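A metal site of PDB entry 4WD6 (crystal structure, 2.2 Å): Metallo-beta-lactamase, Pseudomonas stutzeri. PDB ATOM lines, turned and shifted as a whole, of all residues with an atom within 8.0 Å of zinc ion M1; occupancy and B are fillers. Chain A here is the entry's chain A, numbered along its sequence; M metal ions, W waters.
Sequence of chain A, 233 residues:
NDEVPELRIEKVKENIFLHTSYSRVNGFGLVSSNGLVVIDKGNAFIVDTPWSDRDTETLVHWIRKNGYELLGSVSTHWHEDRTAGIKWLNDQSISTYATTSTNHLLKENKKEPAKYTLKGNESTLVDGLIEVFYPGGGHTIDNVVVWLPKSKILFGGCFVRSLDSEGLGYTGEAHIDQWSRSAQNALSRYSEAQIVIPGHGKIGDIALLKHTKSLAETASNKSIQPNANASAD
Of the 22 residues printed, 3 come within 4 Å of zinc ion M1.
Zinc ion M1 is bound by the side-chain sulfur of Cys 158, a ring nitrogen (NE2) of His 200, the side-chain carboxylate of Asp 81 and water W1. Zinc ion M1 has four donor atoms within binding distance.
NE of Arg 82 sits close to SG of Cys 158 (3.5 Å). The side-chain carboxylate (OD2) of Asp 81 sits close to the guanidinium group (NE) of Arg 82, at 3.0 Å. ND1 of His 200 lies within hydrogen-bond range of O of Ser 32 (2.7 Å).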
ATOM      1  N   VAL A  31      11.836  14.694  -2.291  1.00  0.00           N
ATOM      2  CA  VAL A  31      12.610  13.582  -1.696  1.00  0.00           C
ATOM      3  C   VAL A  31      12.590  13.790  -0.229  1.00  0.00           C
ATOM      4  O   VAL A  31      12.917  14.892   0.235  1.00  0.00           O
ATOM      5  CB  VAL A  31      14.082  13.603  -2.160  1.00  0.00           C
ATOM      6  CG1 VAL A  31      14.896  12.509  -1.481  1.00  0.00           C
ATOM      7  CG2 VAL A  31      14.180  13.465  -3.681  1.00  0.00           C
ATOM      8  N   SER A  32      12.178  12.778   0.524  1.00  0.00           N
ATOM      9  CA  SER A  32      12.264  12.782   1.956  1.00  0.00           C
ATOM     10  C   SER A  32      13.652  12.425   2.489  1.00  0.00           C
ATOM     11  O   SER A  32      14.415  11.715   1.846  1.00  0.00           O
ATOM     12  CB  SER A  32      11.278  11.771   2.522  1.00  0.00           C
ATOM     13  OG  SER A  32      11.629  10.454   2.140  1.00  0.00           O
ATOM     14  N   SER A  33      13.913  12.814   3.730  1.00  0.00           N
ATOM     15  CA  SER A  33      15.232  12.697   4.311  1.00  0.00           C
ATOM     16  C   SER A  33      15.133  12.545   5.835  1.00  0.00           C
ATOM     17  O   SER A  33      14.327  13.240   6.474  1.00  0.00           O
ATOM     18  CB  SER A  33      16.079  13.882   3.908  1.00  0.00           C
ATOM     19  OG  SER A  33      17.412  13.695   4.319  1.00  0.00           O
ATOM     20  N   ASN A  34      15.865  11.580   6.398  1.00  0.00           N
ATOM     21  CA  ASN A  34      15.761  11.246   7.809  1.00  0.00           C
ATOM     22  C   ASN A  34      16.919  11.788   8.665  1.00  0.00           C
ATOM     23  O   ASN A  34      18.075  11.829   8.181  1.00  0.00           O
ATOM     24  CB  ASN A  34      15.701   9.752   8.023  1.00  0.00           C
ATOM     25  CG  ASN A  34      14.565   9.080   7.261  1.00  0.00           C
ATOM     26  OD1 ASN A  34      13.535   9.683   6.994  1.00  0.00           O
ATOM     27  ND2 ASN A  34      14.752   7.804   6.940  1.00  0.00           N
ATOM     28  N   ASP A  48      22.171  14.757  12.095  1.00  0.00           N
ATOM     29  CA  ASP A  48      21.900  15.291  10.744  1.00  0.00           C
ATOM     30  C   ASP A  48      20.878  16.422  10.766  1.00  0.00           C
ATOM     31  O   ASP A  48      19.907  16.403  11.518  1.00  0.00           O
ATOM     32  CB  ASP A  48      21.497  14.186   9.744  1.00  0.00           C
ATOM     33  CG  ASP A  48      22.701  13.386   9.250  1.00  0.00           C
ATOM     34  OD1 ASP A  48      23.756  13.969   9.098  1.00  0.00           O
ATOM     35  OD2 ASP A  48      22.621  12.171   9.021  1.00  0.00           O
ATOM     36  N   TRP A  51      16.841  19.569   5.800  1.00  0.00           N
ATOM     37  CA  TRP A  51      17.309  19.871   4.445  1.00  0.00           C
ATOM     38  C   TRP A  51      17.110  21.353   4.103  1.00  0.00           C
ATOM     39  O   TRP A  51      17.384  21.709   2.962  1.00  0.00           O
ATOM     40  CB  TRP A  51      16.575  18.962   3.399  1.00  0.00           C
ATOM     41  CG  TRP A  51      17.377  18.604   2.170  1.00  0.00           C
ATOM     42  CD1 TRP A  51      18.427  19.320   1.620  1.00  0.00           C
ATOM     43  CD2 TRP A  51      17.173  17.480   1.277  1.00  0.00           C
ATOM     44  NE1 TRP A  51      18.898  18.697   0.496  1.00  0.00           N
ATOM     45  CE2 TRP A  51      18.150  17.573   0.248  1.00  0.00           C
ATOM     46  CE3 TRP A  51      16.276  16.397   1.259  1.00  0.00           C
ATOM     47  CZ2 TRP A  51      18.259  16.613  -0.793  1.00  0.00           C
ATOM     48  CZ3 TRP A  51      16.372  15.451   0.228  1.00  0.00           C
ATOM     49  CH2 TRP A  51      17.359  15.566  -0.782  1.00  0.00           C
ATOM     50  N   THR A  76      26.503  13.256   9.017  1.00  0.00           N
ATOM     51  CA  THR A  76      27.096  11.911   8.686  1.00  0.00           C
ATOM     52  C   THR A  76      27.771  11.736   7.325  1.00  0.00           C
ATOM     53  O   THR A  76      28.387  10.712   7.048  1.00  0.00           O
ATOM     54  CB  THR A  76      26.035  10.812   8.882  1.00  0.00           C
ATOM     55  OG1 THR A  76      24.882  11.050   8.051  1.00  0.00           O
ATOM     56  CG2 THR A  76      25.627  10.749  10.340  1.00  0.00           C
ATOM     57  N   HIS A  77      27.631  12.760   6.491  1.00  0.00           N
ATOM     58  CA  HIS A  77      28.419  13.005   5.288  1.00  0.00           C
ATOM     59  C   HIS A  77      28.067  14.428   4.797  1.00  0.00           C
ATOM     60  O   HIS A  77      27.191  15.098   5.395  1.00  0.00           O
ATOM     61  CB  HIS A  77      28.268  11.895   4.205  1.00  0.00           C
ATOM     62  CG  HIS A  77      26.968  11.900   3.475  1.00  0.00           C
ATOM     63  ND1 HIS A  77      25.827  11.365   4.009  1.00  0.00           N
ATOM     64  CD2 HIS A  77      26.662  12.274   2.216  1.00  0.00           C
ATOM     65  CE1 HIS A  77      24.842  11.478   3.143  1.00  0.00           C
ATOM     66  NE2 HIS A  77      25.332  12.024   2.046  1.00  0.00           N
ATOM     67  N   HIS A  79      26.873  16.041   1.974  1.00  0.00           N
ATOM     68  CA  HIS A  79      25.844  16.518   1.036  1.00  0.00           C
ATOM     69  C   HIS A  79      24.762  17.337   1.756  1.00  0.00           C
ATOM     70  O   HIS A  79      24.567  17.241   2.986  1.00  0.00           O
ATOM     71  CB  HIS A  79      25.215  15.318   0.262  1.00  0.00           C
ATOM     72  CG  HIS A  79      26.153  14.628  -0.677  1.00  0.00           C
ATOM     73  ND1 HIS A  79      26.032  13.295  -1.017  1.00  0.00           N
ATOM     74  CD2 HIS A  79      27.278  15.067  -1.296  1.00  0.00           C
ATOM     75  CE1 HIS A  79      27.015  12.958  -1.836  1.00  0.00           C
ATOM     76  NE2 HIS A  79      27.779  14.008  -2.021  1.00  0.00           N
ATOM     77  N   GLU A  80      24.034  18.124   0.978  1.00  0.00           N
ATOM     78  CA  GLU A  80      23.157  19.126   1.552  1.00  0.00           C
ATOM     79  C   GLU A  80      22.135  18.505   2.498  1.00  0.00           C
ATOM     80  O   GLU A  80      21.815  19.091   3.513  1.00  0.00           O
ATOM     81  CB  GLU A  80      22.417  19.914   0.462  1.00  0.00           C
ATOM     82  CG  GLU A  80      23.302  20.819  -0.398  1.00  0.00           C
ATOM     83  CD  GLU A  80      22.539  21.609  -1.445  1.00  0.00           C
ATOM     84  OE1 GLU A  80      21.280  21.546  -1.430  1.00  0.00           O
ATOM     85  OE2 GLU A  80      23.189  22.297  -2.285  1.00  0.00           O
ATOM     86  N   ASP A  81      21.624  17.318   2.142  1.00  0.00           N
ATOM     87  CA  ASP A  81      20.564  16.683   2.953  1.00  0.00           C
ATOM     88  C   ASP A  81      20.965  16.391   4.408  1.00  0.00           C
ATOM     89  O   ASP A  81      20.116  16.258   5.270  1.00  0.00           O
ATOM     90  CB  ASP A  81      19.938  15.423   2.251  1.00  0.00           C
ATOM     91  CG  ASP A  81      20.954  14.289   2.018  1.00  0.00           C
ATOM     92  OD1 ASP A  81      21.995  14.513   1.389  1.00  0.00           O
ATOM     93  OD2 ASP A  81      20.687  13.154   2.446  1.00  0.00           O
ATOM     94  N   ARG A  82      22.254  16.302   4.659  1.00  0.00           N
ATOM     95  CA  ARG A  82      22.815  16.129   5.986  1.00  0.00           C
ATOM     96  C   ARG A  82      23.298  17.429   6.695  1.00  0.00           C
ATOM     97  O   ARG A  82      23.372  17.481   7.924  1.00  0.00           O
ATOM     98  CB  ARG A  82      24.021  15.210   5.871  1.00  0.00           C
ATOM     99  CG  ARG A  82      23.806  13.886   5.139  1.00  0.00           C
ATOM    100  CD  ARG A  82      22.914  12.965   5.951  1.00  0.00           C
ATOM    101  NE  ARG A  82      21.660  12.711   5.266  1.00  0.00           N
ATOM    102  CZ  ARG A  82      20.549  12.249   5.824  1.00  0.00           C
ATOM    103  NH1 ARG A  82      20.443  11.980   7.111  1.00  0.00           N
ATOM    104  NH2 ARG A  82      19.477  12.059   5.062  1.00  0.00           N
ATOM    105  N   HIS A 139      28.523   5.037  -0.058  1.00  0.00           N
ATOM    106  CA  HIS A 139      27.868   6.187  -0.670  1.00  0.00           C
ATOM    107  C   HIS A 139      28.841   7.321  -0.987  1.00  0.00           C
ATOM    108  O   HIS A 139      28.805   7.871  -2.066  1.00  0.00           O
ATOM    109  CB  HIS A 139      26.831   6.671   0.311  1.00  0.00           C
ATOM    110  CG  HIS A 139      26.195   7.950  -0.087  1.00  0.00           C
ATOM    111  ND1 HIS A 139      25.399   8.049  -1.200  1.00  0.00           N
ATOM    112  CD2 HIS A 139      26.218   9.177   0.472  1.00  0.00           C
ATOM    113  CE1 HIS A 139      24.957   9.288  -1.308  1.00  0.00           C
ATOM    114  NE2 HIS A 139      25.465   9.998  -0.325  1.00  0.00           N
ATOM    115  N   GLY A 157      22.536   6.628   8.185  1.00  0.00           N
ATOM    116  CA  GLY A 157      22.624   7.686   7.189  1.00  0.00           C
ATOM    117  C   GLY A 157      22.428   7.088   5.827  1.00  0.00           C
ATOM    118  O   GLY A 157      21.845   6.008   5.698  1.00  0.00           O
ATOM    119  N   CYS A 158      22.971   7.753   4.820  1.00  0.00           N
ATOM    120  CA  CYS A 158      22.810   7.352   3.425  1.00  0.00           C
ATOM    121  C   CYS A 158      23.794   6.260   3.002  1.00  0.00           C
ATOM    122  O   CYS A 158      23.710   5.753   1.905  1.00  0.00           O
ATOM    123  CB  CYS A 158      22.932   8.579   2.548  1.00  0.00           C
ATOM    124  SG  CYS A 158      21.829   9.928   3.075  1.00  0.00           S
ATOM    125  N   PHE A 159      24.663   5.850   3.927  1.00  0.00           N
ATOM    126  CA  PHE A 159      25.427   4.589   3.823  1.00  0.00           C
ATOM    127  C   PHE A 159      24.573   3.279   3.779  1.00  0.00           C
ATOM    128  O   PHE A 159      25.035   2.244   3.300  1.00  0.00           O
ATOM    129  CB  PHE A 159      26.441   4.567   4.985  1.00  0.00           C
ATOM    130  CG  PHE A 159      27.273   3.334   5.022  1.00  0.00           C
ATOM    131  CD1 PHE A 159      26.978   2.316   5.912  1.00  0.00           C
ATOM    132  CD2 PHE A 159      28.405   3.221   4.225  1.00  0.00           C
ATOM    133  CE1 PHE A 159      27.758   1.160   5.943  1.00  0.00           C
ATOM    134  CE2 PHE A 159      29.178   2.071   4.256  1.00  0.00           C
ATOM    135  CZ  PHE A 159      28.850   1.037   5.111  1.00  0.00           C
ATOM    136  N   VAL A 160      23.336   3.384   4.257  1.00  0.00           N
ATOM    137  CA  VAL A 160      22.369   2.319   4.358  1.00  0.00           C
ATOM    138  C   VAL A 160      21.088   2.654   3.551  1.00  0.00           C
ATOM    139  O   VAL A 160      20.559   3.757   3.631  1.00  0.00           O
ATOM    140  CB  VAL A 160      21.949   2.129   5.824  1.00  0.00           C
ATOM    141  CG1 VAL A 160      20.864   1.069   5.950  1.00  0.00           C
ATOM    142  CG2 VAL A 160      23.157   1.759   6.673  1.00  0.00           C
ATOM    143  N   ARG A 161      20.616   1.685   2.806  1.00  0.00           N
ATOM    144  CA  ARG A 161      19.484   1.864   1.915  1.00  0.00           C
ATOM    145  C   ARG A 161      18.337   1.237   2.606  1.00  0.00           C
ATOM    146  O   ARG A 161      18.529   0.326   3.418  1.00  0.00           O
ATOM    147  CB  ARG A 161      19.768   1.199   0.555  1.00  0.00           C
ATOM    148  CG  ARG A 161      21.022   1.774  -0.096  1.00  0.00           C
ATOM    149  CD  ARG A 161      20.827   3.248  -0.469  1.00  0.00           C
ATOM    150  NE  ARG A 161      19.775   3.318  -1.476  1.00  0.00           N
ATOM    151  CZ  ARG A 161      19.085   4.407  -1.808  1.00  0.00           C
ATOM    152  NH1 ARG A 161      19.326   5.602  -1.276  1.00  0.00           N
ATOM    153  NH2 ARG A 161      18.160   4.298  -2.744  1.00  0.00           N
ATOM    154  N   TYR A 170      22.245   7.882  -5.791  1.00  0.00           N
ATOM    155  CA  TYR A 170      23.301   8.606  -6.514  1.00  0.00           C
ATOM    156  C   TYR A 170      24.679   7.970  -6.200  1.00  0.00           C
ATOM    157  O   TYR A 170      25.101   7.928  -5.042  1.00  0.00           O
ATOM    158  CB  TYR A 170      23.260  10.133  -6.192  1.00  0.00           C
ATOM    159  CG  TYR A 170      24.510  10.868  -6.568  1.00  0.00           C
ATOM    160  CD1 TYR A 170      24.738  11.307  -7.888  1.00  0.00           C
ATOM    161  CD2 TYR A 170      25.500  11.127  -5.617  1.00  0.00           C
ATOM    162  CE1 TYR A 170      25.900  11.977  -8.239  1.00  0.00           C
ATOM    163  CE2 TYR A 170      26.670  11.790  -5.959  1.00  0.00           C
ATOM    164  CZ  TYR A 170      26.871  12.230  -7.265  1.00  0.00           C
ATOM    165  OH  TYR A 170      28.045  12.866  -7.586  1.00  0.00           O
ATOM    166  N   PRO A 198      17.847   4.212   7.948  1.00  0.00           N
ATOM    167  CA  PRO A 198      18.497   4.716   6.762  1.00  0.00           C
ATOM    168  C   PRO A 198      18.298   6.226   6.581  1.00  0.00           C
ATOM    169  O   PRO A 198      17.425   6.821   7.243  1.00  0.00           O
ATOM    170  CB  PRO A 198      17.758   3.982   5.649  1.00  0.00           C
ATOM    171  CG  PRO A 198      16.350   3.936   6.166  1.00  0.00           C
ATOM    172  CD  PRO A 198      16.489   3.745   7.650  1.00  0.00           C
ATOM    173  N   GLY A 199      19.096   6.801   5.665  1.00  0.00           N
ATOM    174  CA  GLY A 199      19.062   8.247   5.374  1.00  0.00           C
ATOM    175  C   GLY A 199      17.778   8.736   4.721  1.00  0.00           C
ATOM    176  O   GLY A 199      17.399   9.897   4.921  1.00  0.00           O
ATOM    177  N   HIS A 200      17.178   7.827   3.940  1.00  0.00           N
ATOM    178  CA  HIS A 200      15.947   8.023   3.162  1.00  0.00           C
ATOM    179  C   HIS A 200      15.127   6.758   3.324  1.00  0.00           C
ATOM    180  O   HIS A 200      15.641   5.660   3.184  1.00  0.00           O
ATOM    181  CB  HIS A 200      16.296   8.212   1.706  1.00  0.00           C
ATOM    182  CG  HIS A 200      17.261   9.314   1.482  1.00  0.00           C
ATOM    183  ND1 HIS A 200      16.872  10.643   1.464  1.00  0.00           N
ATOM    184  CD2 HIS A 200      18.608   9.319   1.369  1.00  0.00           C
ATOM    185  CE1 HIS A 200      17.946  11.404   1.322  1.00  0.00           C
ATOM    186  NE2 HIS A 200      19.001  10.616   1.211  1.00  0.00           N
HETATM  187 ZN    ZN M   1      21.170  11.140   1.402  1.00  0.00          ZN
HETATM  188 ZN    ZN M   2      24.696  11.960  -0.220  1.00  0.00          ZN
HETATM  189  O   HOH W   1      22.894  12.097  -0.024  1.00  0.00           O
